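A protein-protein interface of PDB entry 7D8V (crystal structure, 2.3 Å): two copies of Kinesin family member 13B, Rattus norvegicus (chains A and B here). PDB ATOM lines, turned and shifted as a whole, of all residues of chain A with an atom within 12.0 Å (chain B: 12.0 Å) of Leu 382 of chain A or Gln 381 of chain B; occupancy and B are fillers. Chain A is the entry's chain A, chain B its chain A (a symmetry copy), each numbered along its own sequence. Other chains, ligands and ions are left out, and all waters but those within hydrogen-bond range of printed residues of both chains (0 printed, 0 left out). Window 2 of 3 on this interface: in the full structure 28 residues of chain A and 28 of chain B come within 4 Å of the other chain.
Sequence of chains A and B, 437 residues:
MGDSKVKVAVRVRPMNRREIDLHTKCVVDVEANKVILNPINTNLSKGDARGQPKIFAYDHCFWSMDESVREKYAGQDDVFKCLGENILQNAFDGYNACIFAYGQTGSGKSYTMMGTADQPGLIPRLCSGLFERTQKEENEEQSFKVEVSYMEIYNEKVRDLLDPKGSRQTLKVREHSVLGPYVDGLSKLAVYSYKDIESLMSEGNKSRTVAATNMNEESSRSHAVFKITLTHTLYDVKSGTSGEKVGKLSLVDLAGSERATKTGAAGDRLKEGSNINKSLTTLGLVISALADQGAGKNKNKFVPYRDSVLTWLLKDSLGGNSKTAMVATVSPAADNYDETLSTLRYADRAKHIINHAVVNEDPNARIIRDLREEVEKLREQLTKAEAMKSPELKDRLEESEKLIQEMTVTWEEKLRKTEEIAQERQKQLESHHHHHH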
ATOM      1  N   GLU A 373      20.481   9.661 -20.331  1.00  0.00           N
ATOM      2  CA  GLU A 373      21.122   9.905 -21.619  1.00  0.00           C
ATOM      3  C   GLU A 373      22.415   9.100 -21.748  1.00  0.00           C
ATOM      4  O   GLU A 373      22.691   8.519 -22.802  1.00  0.00           O
ATOM      5  CB  GLU A 373      21.385  11.404 -21.804  1.00  0.00           C
ATOM      6  CG  GLU A 373      22.191  11.754 -23.065  1.00  0.00           C
ATOM      7  CD  GLU A 373      22.376  13.263 -23.264  1.00  0.00           C
ATOM      8  OE1 GLU A 373      21.868  13.809 -24.271  1.00  0.00           O
ATOM      9  OE2 GLU A 373      23.023  13.902 -22.400  1.00  0.00           O
ATOM     10  N   GLU A 374      23.221   9.053 -20.685  1.00  0.00           N
ATOM     11  CA  GLU A 374      24.452   8.276 -20.743  1.00  0.00           C
ATOM     12  C   GLU A 374      24.153   6.794 -20.896  1.00  0.00           C
ATOM     13  O   GLU A 374      24.866   6.077 -21.604  1.00  0.00           O
ATOM     14  CB  GLU A 374      25.310   8.531 -19.504  1.00  0.00           C
ATOM     15  CG  GLU A 374      26.676   7.856 -19.580  1.00  0.00           C
ATOM     16  CD  GLU A 374      27.749   8.597 -18.793  1.00  0.00           C
ATOM     17  OE1 GLU A 374      27.442   9.681 -18.244  1.00  0.00           O
ATOM     18  OE2 GLU A 374      28.901   8.104 -18.735  1.00  0.00           O
ATOM     19  N   VAL A 375      23.088   6.319 -20.251  1.00  0.00           N
ATOM     20  CA  VAL A 375      22.692   4.926 -20.422  1.00  0.00           C
ATOM     21  C   VAL A 375      22.347   4.647 -21.878  1.00  0.00           C
ATOM     22  O   VAL A 375      22.744   3.619 -22.435  1.00  0.00           O
ATOM     23  CB  VAL A 375      21.517   4.584 -19.485  1.00  0.00           C
ATOM     24  CG1 VAL A 375      20.774   3.340 -19.979  1.00  0.00           C
ATOM     25  CG2 VAL A 375      22.014   4.400 -18.059  1.00  0.00           C
ATOM     26  N   GLU A 376      21.606   5.552 -22.520  1.00  0.00           N
ATOM     27  CA  GLU A 376      21.243   5.319 -23.918  1.00  0.00           C
ATOM     28  C   GLU A 376      22.462   5.376 -24.837  1.00  0.00           C
ATOM     29  O   GLU A 376      22.590   4.560 -25.766  1.00  0.00           O
ATOM     30  CB  GLU A 376      20.178   6.320 -24.363  1.00  0.00           C
ATOM     31  CG  GLU A 376      18.871   6.152 -23.623  1.00  0.00           C
ATOM     32  CD  GLU A 376      18.292   4.766 -23.812  1.00  0.00           C
ATOM     33  OE1 GLU A 376      17.909   4.147 -22.793  1.00  0.00           O
ATOM     34  OE2 GLU A 376      18.236   4.290 -24.972  1.00  0.00           O
ATOM     35  N   LYS A 377      23.363   6.334 -24.599  1.00  0.00           N
ATOM     36  CA  LYS A 377      24.602   6.403 -25.373  1.00  0.00           C
ATOM     37  C   LYS A 377      25.387   5.102 -25.255  1.00  0.00           C
ATOM     38  O   LYS A 377      25.794   4.512 -26.264  1.00  0.00           O
ATOM     39  CB  LYS A 377      25.448   7.591 -24.914  1.00  0.00           C
ATOM     40  N   LEU A 378      25.581   4.621 -24.023  1.00  0.00           N
ATOM     41  CA  LEU A 378      26.280   3.356 -23.831  1.00  0.00           C
ATOM     42  C   LEU A 378      25.544   2.205 -24.510  1.00  0.00           C
ATOM     43  O   LEU A 378      26.172   1.355 -25.152  1.00  0.00           O
ATOM     44  CB  LEU A 378      26.466   3.083 -22.337  1.00  0.00           C
ATOM     45  CG  LEU A 378      27.323   4.128 -21.614  1.00  0.00           C
ATOM     46  CD1 LEU A 378      27.517   3.804 -20.137  1.00  0.00           C
ATOM     47  CD2 LEU A 378      28.665   4.259 -22.306  1.00  0.00           C
ATOM     48  N   ARG A 379      24.212   2.164 -24.395  1.00  0.00           N
ATOM     49  CA  ARG A 379      23.459   1.040 -24.949  1.00  0.00           C
ATOM     50  C   ARG A 379      23.632   0.952 -26.456  1.00  0.00           C
ATOM     51  O   ARG A 379      23.765  -0.146 -27.009  1.00  0.00           O
ATOM     52  CB  ARG A 379      21.975   1.157 -24.590  1.00  0.00           C
ATOM     53  CG  ARG A 379      21.600   0.533 -23.250  1.00  0.00           C
ATOM     54  CD  ARG A 379      20.103   0.632 -22.975  1.00  0.00           C
ATOM     55  NE  ARG A 379      19.758   0.164 -21.632  1.00  0.00           N
ATOM     56  CZ  ARG A 379      18.711   0.593 -20.929  1.00  0.00           C
ATOM     57  NH1 ARG A 379      17.895   1.511 -21.433  1.00  0.00           N
ATOM     58  NH2 ARG A 379      18.482   0.107 -19.714  1.00  0.00           N
ATOM     59  N   GLU A 380      23.640   2.095 -27.145  1.00  0.00           N
ATOM     60  CA  GLU A 380      23.819   2.013 -28.588  1.00  0.00           C
ATOM     61  C   GLU A 380      25.285   1.884 -28.994  1.00  0.00           C
ATOM     62  O   GLU A 380      25.565   1.376 -30.084  1.00  0.00           O
ATOM     63  CB  GLU A 380      23.160   3.204 -29.284  1.00  0.00           C
ATOM     64  CG  GLU A 380      23.869   4.529 -29.150  1.00  0.00           C
ATOM     65  CD  GLU A 380      23.520   5.465 -30.294  1.00  0.00           C
ATOM     66  OE1 GLU A 380      22.315   5.606 -30.597  1.00  0.00           O
ATOM     67  OE2 GLU A 380      24.446   6.055 -30.892  1.00  0.00           O
ATOM     68  N   GLN A 381      26.227   2.308 -28.147  1.00  0.00           N
ATOM     69  CA  GLN A 381      27.623   1.952 -28.390  1.00  0.00           C
ATOM     70  C   GLN A 381      27.807   0.444 -28.331  1.00  0.00           C
ATOM     71  O   GLN A 381      28.526  -0.139 -29.152  1.00  0.00           O
ATOM     72  CB  GLN A 381      28.535   2.632 -27.372  1.00  0.00           C
ATOM     73  CG  GLN A 381      28.907   4.064 -27.709  1.00  0.00           C
ATOM     74  CD  GLN A 381      29.853   4.670 -26.688  1.00  0.00           C
ATOM     75  OE1 GLN A 381      29.794   4.342 -25.503  1.00  0.00           O
ATOM     76  NE2 GLN A 381      30.738   5.551 -27.146  1.00  0.00           N
ATOM     77  N   LEU A 382      27.145  -0.204 -27.366  1.00  0.00           N
ATOM     78  CA  LEU A 382      27.214  -1.656 -27.220  1.00  0.00           C
ATOM     79  C   LEU A 382      26.735  -2.381 -28.473  1.00  0.00           C
ATOM     80  O   LEU A 382      27.129  -3.526 -28.719  1.00  0.00           O
ATOM     81  CB  LEU A 382      26.385  -2.087 -26.010  1.00  0.00           C
ATOM     82  CG  LEU A 382      26.414  -3.566 -25.635  1.00  0.00           C
ATOM     83  CD1 LEU A 382      27.402  -3.830 -24.507  1.00  0.00           C
ATOM     84  CD2 LEU A 382      25.012  -4.041 -25.273  1.00  0.00           C
ATOM     85  N   THR A 383      25.885  -1.747 -29.268  1.00  0.00           N
ATOM     86  CA  THR A 383      25.452  -2.322 -30.536  1.00  0.00           C
ATOM     87  C   THR A 383      26.579  -2.104 -31.541  1.00  0.00           C
ATOM     88  O   THR A 383      26.643  -1.092 -32.238  1.00  0.00           O
ATOM     89  CB  THR A 383      24.148  -1.689 -30.993  1.00  0.00           C
ATOM     90  OG1 THR A 383      23.161  -1.855 -29.965  1.00  0.00           O
ATOM     91  CG2 THR A 383      23.658  -2.359 -32.279  1.00  0.00           C
ATOM     92  N   LYS A 384      27.493  -3.066 -31.597  1.00  0.00           N
ATOM     93  CA  LYS A 384      28.654  -2.989 -32.477  1.00  0.00           C
ATOM     94  C   LYS A 384      29.274  -4.374 -32.644  1.00  0.00           C
ATOM     95  O   LYS A 384      29.074  -5.252 -31.804  1.00  0.00           O
ATOM     96  CB  LYS A 384      29.684  -2.001 -31.922  1.00  0.00           C
ATOM     97  N   ASP B 370      20.649   3.364  -8.801  1.00  0.00           N
ATOM     98  CA  ASP B 370      20.433   2.289  -9.766  1.00  0.00           C
ATOM     99  C   ASP B 370      20.984   2.667 -11.135  1.00  0.00           C
ATOM    100  O   ASP B 370      21.569   1.830 -11.833  1.00  0.00           O
ATOM    101  CB  ASP B 370      18.943   1.943  -9.852  1.00  0.00           C
ATOM    102  CG  ASP B 370      18.434   1.258  -8.597  1.00  0.00           C
ATOM    103  OD1 ASP B 370      17.202   1.092  -8.454  1.00  0.00           O
ATOM    104  OD2 ASP B 370      19.277   0.893  -7.744  1.00  0.00           O
ATOM    105  N   LEU B 371      20.828   3.932 -11.531  1.00  0.00           N
ATOM    106  CA  LEU B 371      21.315   4.346 -12.842  1.00  0.00           C
ATOM    107  C   LEU B 371      22.839   4.367 -12.890  1.00  0.00           C
ATOM    108  O   LEU B 371      23.439   4.026 -13.915  1.00  0.00           O
ATOM    109  CB  LEU B 371      20.736   5.718 -13.188  1.00  0.00           C
ATOM    110  CG  LEU B 371      19.313   5.689 -13.746  1.00  0.00           C
ATOM    111  CD1 LEU B 371      18.718   7.090 -13.791  1.00  0.00           C
ATOM    112  CD2 LEU B 371      19.313   5.068 -15.141  1.00  0.00           C
ATOM    113  N   ARG B 372      23.485   4.764 -11.796  1.00  0.00           N
ATOM    114  CA  ARG B 372      24.945   4.722 -11.760  1.00  0.00           C
ATOM    115  C   ARG B 372      25.441   3.285 -11.821  1.00  0.00           C
ATOM    116  O   ARG B 372      26.432   2.985 -12.505  1.00  0.00           O
ATOM    117  CB  ARG B 372      25.464   5.410 -10.499  1.00  0.00           C
ATOM    118  CG  ARG B 372      25.180   6.902 -10.429  1.00  0.00           C
ATOM    119  CD  ARG B 372      26.343   7.641  -9.800  1.00  0.00           C
ATOM    120  NE  ARG B 372      26.253   9.075 -10.045  1.00  0.00           N
ATOM    121  CZ  ARG B 372      25.909   9.959  -9.121  1.00  0.00           C
ATOM    122  NH1 ARG B 372      25.642   9.551  -7.892  1.00  0.00           N
ATOM    123  NH2 ARG B 372      25.841  11.246  -9.424  1.00  0.00           N
ATOM    124  N   GLU B 373      24.749   2.378 -11.124  1.00  0.00           N
ATOM    125  CA  GLU B 373      25.104   0.965 -11.221  1.00  0.00           C
ATOM    126  C   GLU B 373      24.933   0.456 -12.652  1.00  0.00           C
ATOM    127  O   GLU B 373      25.781  -0.282 -13.162  1.00  0.00           O
ATOM    128  CB  GLU B 373      24.268   0.140 -10.238  1.00  0.00           C
ATOM    129  CG  GLU B 373      24.458  -1.380 -10.364  1.00  0.00           C
ATOM    130  CD  GLU B 373      23.667  -2.176  -9.321  1.00  0.00           C
ATOM    131  OE1 GLU B 373      24.292  -2.861  -8.477  1.00  0.00           O
ATOM    132  OE2 GLU B 373      22.414  -2.106  -9.343  1.00  0.00           O
ATOM    133  N   GLU B 374      23.840   0.839 -13.316  1.00  0.00           N
ATOM    134  CA  GLU B 374      23.640   0.406 -14.693  1.00  0.00           C
ATOM    135  C   GLU B 374      24.705   0.990 -15.606  1.00  0.00           C
ATOM    136  O   GLU B 374      25.169   0.325 -16.537  1.00  0.00           O
ATOM    137  CB  GLU B 374      22.241   0.785 -15.180  1.00  0.00           C
ATOM    138  CG  GLU B 374      21.924   0.229 -16.564  1.00  0.00           C
ATOM    139  CD  GLU B 374      20.438  -0.027 -16.776  1.00  0.00           C
ATOM    140  OE1 GLU B 374      19.659   0.163 -15.814  1.00  0.00           O
ATOM    141  OE2 GLU B 374      20.051  -0.432 -17.899  1.00  0.00           O
ATOM    142  N   VAL B 375      25.118   2.229 -15.345  1.00  0.00           N
ATOM    143  CA  VAL B 375      26.199   2.820 -16.126  1.00  0.00           C
ATOM    144  C   VAL B 375      27.476   2.005 -15.966  1.00  0.00           C
ATOM    145  O   VAL B 375      28.181   1.740 -16.944  1.00  0.00           O
ATOM    146  CB  VAL B 375      26.410   4.292 -15.722  1.00  0.00           C
ATOM    147  CG1 VAL B 375      27.804   4.771 -16.134  1.00  0.00           C
ATOM    148  CG2 VAL B 375      25.323   5.167 -16.328  1.00  0.00           C
ATOM    149  N   GLU B 376      27.795   1.595 -14.738  1.00  0.00           N
ATOM    150  CA  GLU B 376      29.018   0.819 -14.537  1.00  0.00           C
ATOM    151  C   GLU B 376      28.926  -0.561 -15.187  1.00  0.00           C
ATOM    152  O   GLU B 376      29.901  -1.039 -15.792  1.00  0.00           O
ATOM    153  CB  GLU B 376      29.331   0.699 -13.046  1.00  0.00           C
ATOM    154  CG  GLU B 376      29.646   2.031 -12.406  1.00  0.00           C
ATOM    155  CD  GLU B 376      30.833   2.704 -13.062  1.00  0.00           C
ATOM    156  OE1 GLU B 376      30.717   3.909 -13.388  1.00  0.00           O
ATOM    157  OE2 GLU B 376      31.871   2.029 -13.268  1.00  0.00           O
ATOM    158  N   LYS B 377      27.768  -1.218 -15.067  1.00  0.00           N
ATOM    159  CA  LYS B 377      27.566  -2.502 -15.735  1.00  0.00           C
ATOM    160  C   LYS B 377      27.776  -2.369 -17.239  1.00  0.00           C
ATOM    161  O   LYS B 377      28.531  -3.141 -17.846  1.00  0.00           O
ATOM    162  CB  LYS B 377      26.170  -3.045 -15.429  1.00  0.00           C
ATOM    163  N   LEU B 378      27.139  -1.369 -17.854  1.00  0.00           N
ATOM    164  CA  LEU B 378      27.329  -1.146 -19.283  1.00  0.00           C
ATOM    165  C   LEU B 378      28.788  -0.842 -19.610  1.00  0.00           C
ATOM    166  O   LEU B 378      29.328  -1.363 -20.593  1.00  0.00           O
ATOM    167  CB  LEU B 378      26.414  -0.017 -19.761  1.00  0.00           C
ATOM    168  CG  LEU B 378      24.918  -0.314 -19.597  1.00  0.00           C
ATOM    169  CD1 LEU B 378      24.037   0.816 -20.118  1.00  0.00           C
ATOM    170  CD2 LEU B 378      24.575  -1.615 -20.293  1.00  0.00           C
ATOM    171  N   ARG B 379      29.450  -0.016 -18.793  1.00  0.00           N
ATOM    172  CA  ARG B 379      30.823   0.381 -19.101  1.00  0.00           C
ATOM    173  C   ARG B 379      31.750  -0.823 -19.126  1.00  0.00           C
ATOM    174  O   ARG B 379      32.633  -0.916 -19.987  1.00  0.00           O
ATOM    175  CB  ARG B 379      31.323   1.418 -18.092  1.00  0.00           C
ATOM    176  CG  ARG B 379      30.999   2.862 -18.459  1.00  0.00           C
ATOM    177  CD  ARG B 379      31.570   3.848 -17.446  1.00  0.00           C
ATOM    178  NE  ARG B 379      31.143   5.222 -17.714  1.00  0.00           N
ATOM    179  CZ  ARG B 379      31.018   6.169 -16.786  1.00  0.00           C
ATOM    180  NH1 ARG B 379      31.281   5.899 -15.513  1.00  0.00           N
ATOM    181  NH2 ARG B 379      30.621   7.389 -17.130  1.00  0.00           N
ATOM    182  N   GLU B 380      31.569  -1.762 -18.195  1.00  0.00           N
ATOM    183  CA  GLU B 380      32.450  -2.922 -18.226  1.00  0.00           C
ATOM    184  C   GLU B 380      31.994  -3.980 -19.228  1.00  0.00           C
ATOM    185  O   GLU B 380      32.825  -4.774 -19.683  1.00  0.00           O
ATOM    186  CB  GLU B 380      32.604  -3.521 -16.828  1.00  0.00           C
ATOM    187  CG  GLU B 380      31.416  -4.285 -16.296  1.00  0.00           C
ATOM    188  CD  GLU B 380      31.832  -5.300 -15.246  1.00  0.00           C
ATOM    189  OE1 GLU B 380      32.598  -4.924 -14.331  1.00  0.00           O
ATOM    190  OE2 GLU B 380      31.401  -6.470 -15.335  1.00  0.00           O
ATOM    191  N   GLN B 381      30.713  -4.005 -19.602  1.00  0.00           N
ATOM    192  CA  GLN B 381      30.315  -4.819 -20.747  1.00  0.00           C
ATOM    193  C   GLN B 381      30.998  -4.329 -22.014  1.00  0.00           C
ATOM    194  O   GLN B 381      31.460  -5.131 -22.835  1.00  0.00           O
ATOM    195  CB  GLN B 381      28.799  -4.791 -20.925  1.00  0.00           C
ATOM    196  CG  GLN B 381      28.037  -5.767 -20.046  1.00  0.00           C
ATOM    197  CD  GLN B 381      26.542  -5.727 -20.302  1.00  0.00           C
ATOM    198  OE1 GLN B 381      25.987  -4.680 -20.634  1.00  0.00           O
ATOM    199  NE2 GLN B 381      25.884  -6.875 -20.160  1.00  0.00           N
ATOM    200  N   LEU B 382      31.084  -3.004 -22.176  1.00  0.00           N
ATOM    201  CA  LEU B 382      31.742  -2.406 -23.334  1.00  0.00           C
ATOM    202  C   LEU B 382      33.201  -2.831 -23.447  1.00  0.00           C
ATOM    203  O   LEU B 382      33.772  -2.817 -24.542  1.00  0.00           O
ATOM    204  CB  LEU B 382      31.640  -0.883 -23.249  1.00  0.00           C
ATOM    205  CG  LEU B 382      32.187  -0.080 -24.426  1.00  0.00           C
ATOM    206  CD1 LEU B 382      31.072   0.332 -25.378  1.00  0.00           C
ATOM    207  CD2 LEU B 382      32.964   1.129 -23.917  1.00  0.00           C
ATOM    208  N   THR B 383      33.825  -3.200 -22.337  1.00  0.00           N
ATOM    209  CA  THR B 383      35.189  -3.716 -22.363  1.00  0.00           C
ATOM    210  C   THR B 383      35.115  -5.169 -22.823  1.00  0.00           C
ATOM    211  O   THR B 383      34.979  -6.098 -22.027  1.00  0.00           O
ATOM    212  CB  THR B 383      35.839  -3.582 -20.996  1.00  0.00           C
ATOM    213  OG1 THR B 383      35.795  -2.207 -20.589  1.00  0.00           O
ATOM    214  CG2 THR B 383      37.296  -4.047 -21.055  1.00  0.00           C
ATOM    215  N   LYS B 384      35.184  -5.361 -24.135  1.00  0.00           N
ATOM    216  CA  LYS B 384      35.087  -6.687 -24.736  1.00  0.00           C
ATOM    217  C   LYS B 384      35.616  -6.649 -26.168  1.00  0.00           C
ATOM    218  O   LYS B 384      35.659  -5.588 -26.789  1.00  0.00           O
ATOM    219  CB  LYS B 384      33.640  -7.185 -24.710  1.00  0.00           C
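The guanidinium group (NH2) of Arg 379 of chain A is in salt-bridge range of the side-chain carboxylate (OE2) of Glu 374 of chain B (2.5 Å).
OE2 of Glu 374 of chain A is in salt-bridge range of NH2 of Arg 379 of chain B (2.5 Å).
The side-chain hydroxyl (OG1) of Thr 383 of chain A is in hydrogen-bond range of the backbone carbonyl oxygen (O) of Arg 379 of chain A, at 3.5 Å.
O of Arg 379 of chain B is in hydrogen-bond range of OG1 of Thr 383 of chain B, 3.5 Å away.
The guanidinium group of Arg 379 of chain A is in salt-bridge range of the side-chain carboxylate of Glu 376 of chain A.
The side-chain carboxylate (OE1) of Glu 376 of chain B lies within salt-bridge range of the guanidinium group (NH1) of Arg 379 of chain B, 3.0 Å away.
Among the printed residues, pairs that only touch across the chains: Val 375 of chain A with Val 375 of chain B (3.8 Å), Leu 378 of chain A with Val 375 of chain B (3.9 Å), Val 375 of chain A with Leu 378 of chain B (3.9 Å), Gln 381 of chain A with Leu 382 of chain B (3.96 Å), Leu 382 of chain A with Gln 381 of chain B (3.96 Å), Leu 378 of chain A with Arg 379 of chain B (3.98 Å), Arg 379 of chain A with Leu 378 of chain B (3.98 Å) and Leu 378 of chain A with Leu 378 of chain B (3.99 Å).
Of the printed residues of chain B, Val 375 of chain A touches Val 375 and Leu 378.
Of the printed residues of chain B, Leu 378 of chain A touches Val 375 (3.9 Å), Leu 378 (3.99 Å) and Arg 379 (3.98 Å).
Of chain B, only Gln 381 comes within 4 Å of Leu 382 of chain A.
No residue of chain B comes within 4 Å of Thr 383 of chain A.
Printed residues of chain A within 4 Å of Glu 374 of chain B: Arg 379 (2.5 Å).
Printed residues of chain A within 4 Å of Val 375 of chain B: Val 375 (3.8 Å) and Leu 378 (3.9 Å).
No residue of chain A comes within 4 Å of Lys 377 of chain B.
Printed residues of chain A within 4 Å of Arg 379 of chain B: Glu 374 and Leu 378.
No residue of chain A comes within 4 Å of Glu 380 of chain B.
Of chain A, only Leu 382 comes within 4 Å of Gln 381 of chain B.
Leu 382 of chain B touches one residue of chain A.
No residue of chain A comes within 4 Å of Lys 384 of chain B.
The nearest residue of chain B that does not touch Leu 382 of chain A is Leu 382 of chain B (4.4 Å).
The nearest residue of chain A that does not touch Gln 381 of chain B is Arg 379 of chain A (7.3 Å).
The nearest printed residue of chain A that does not touch Val 375 of chain B is Glu 374 of chain A (4.4 Å).
Of the 15 printed residues of chain B, 6 touch a printed residue of chain A.
Printed residues of chain A that touch a printed residue of chain B: Glu 374, Val 375, Leu 378, Arg 379, Gln 381 and Leu 382.
Hydrophobic or aromatic side chains of chain A that line the printed part of chain B: Val 375, Leu 378 and Leu 382.
Among the printed residues, 10 pairs touch across the chains.
Glu 374 of chain A touches Arg 379 of chain B, and with the chains exchanged Arg 379 of chain A touches Glu 374 of chain B.
Val 375 of chain A touches Leu 378 of chain B, and with the chains exchanged Leu 378 of chain A touches Val 375 of chain B.
Leu 378 of chain B touches its own counterpart, Leu 378 of chain A.
Gln 381 of chain A touches Leu 382 of chain B, and with the chains exchanged Leu 382 of chain A touches Gln 381 of chain B.
Positions printed for both chains: 373, 374, 375, 376, 377, 378, 379, 380, 381, 382, 383 and 384.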
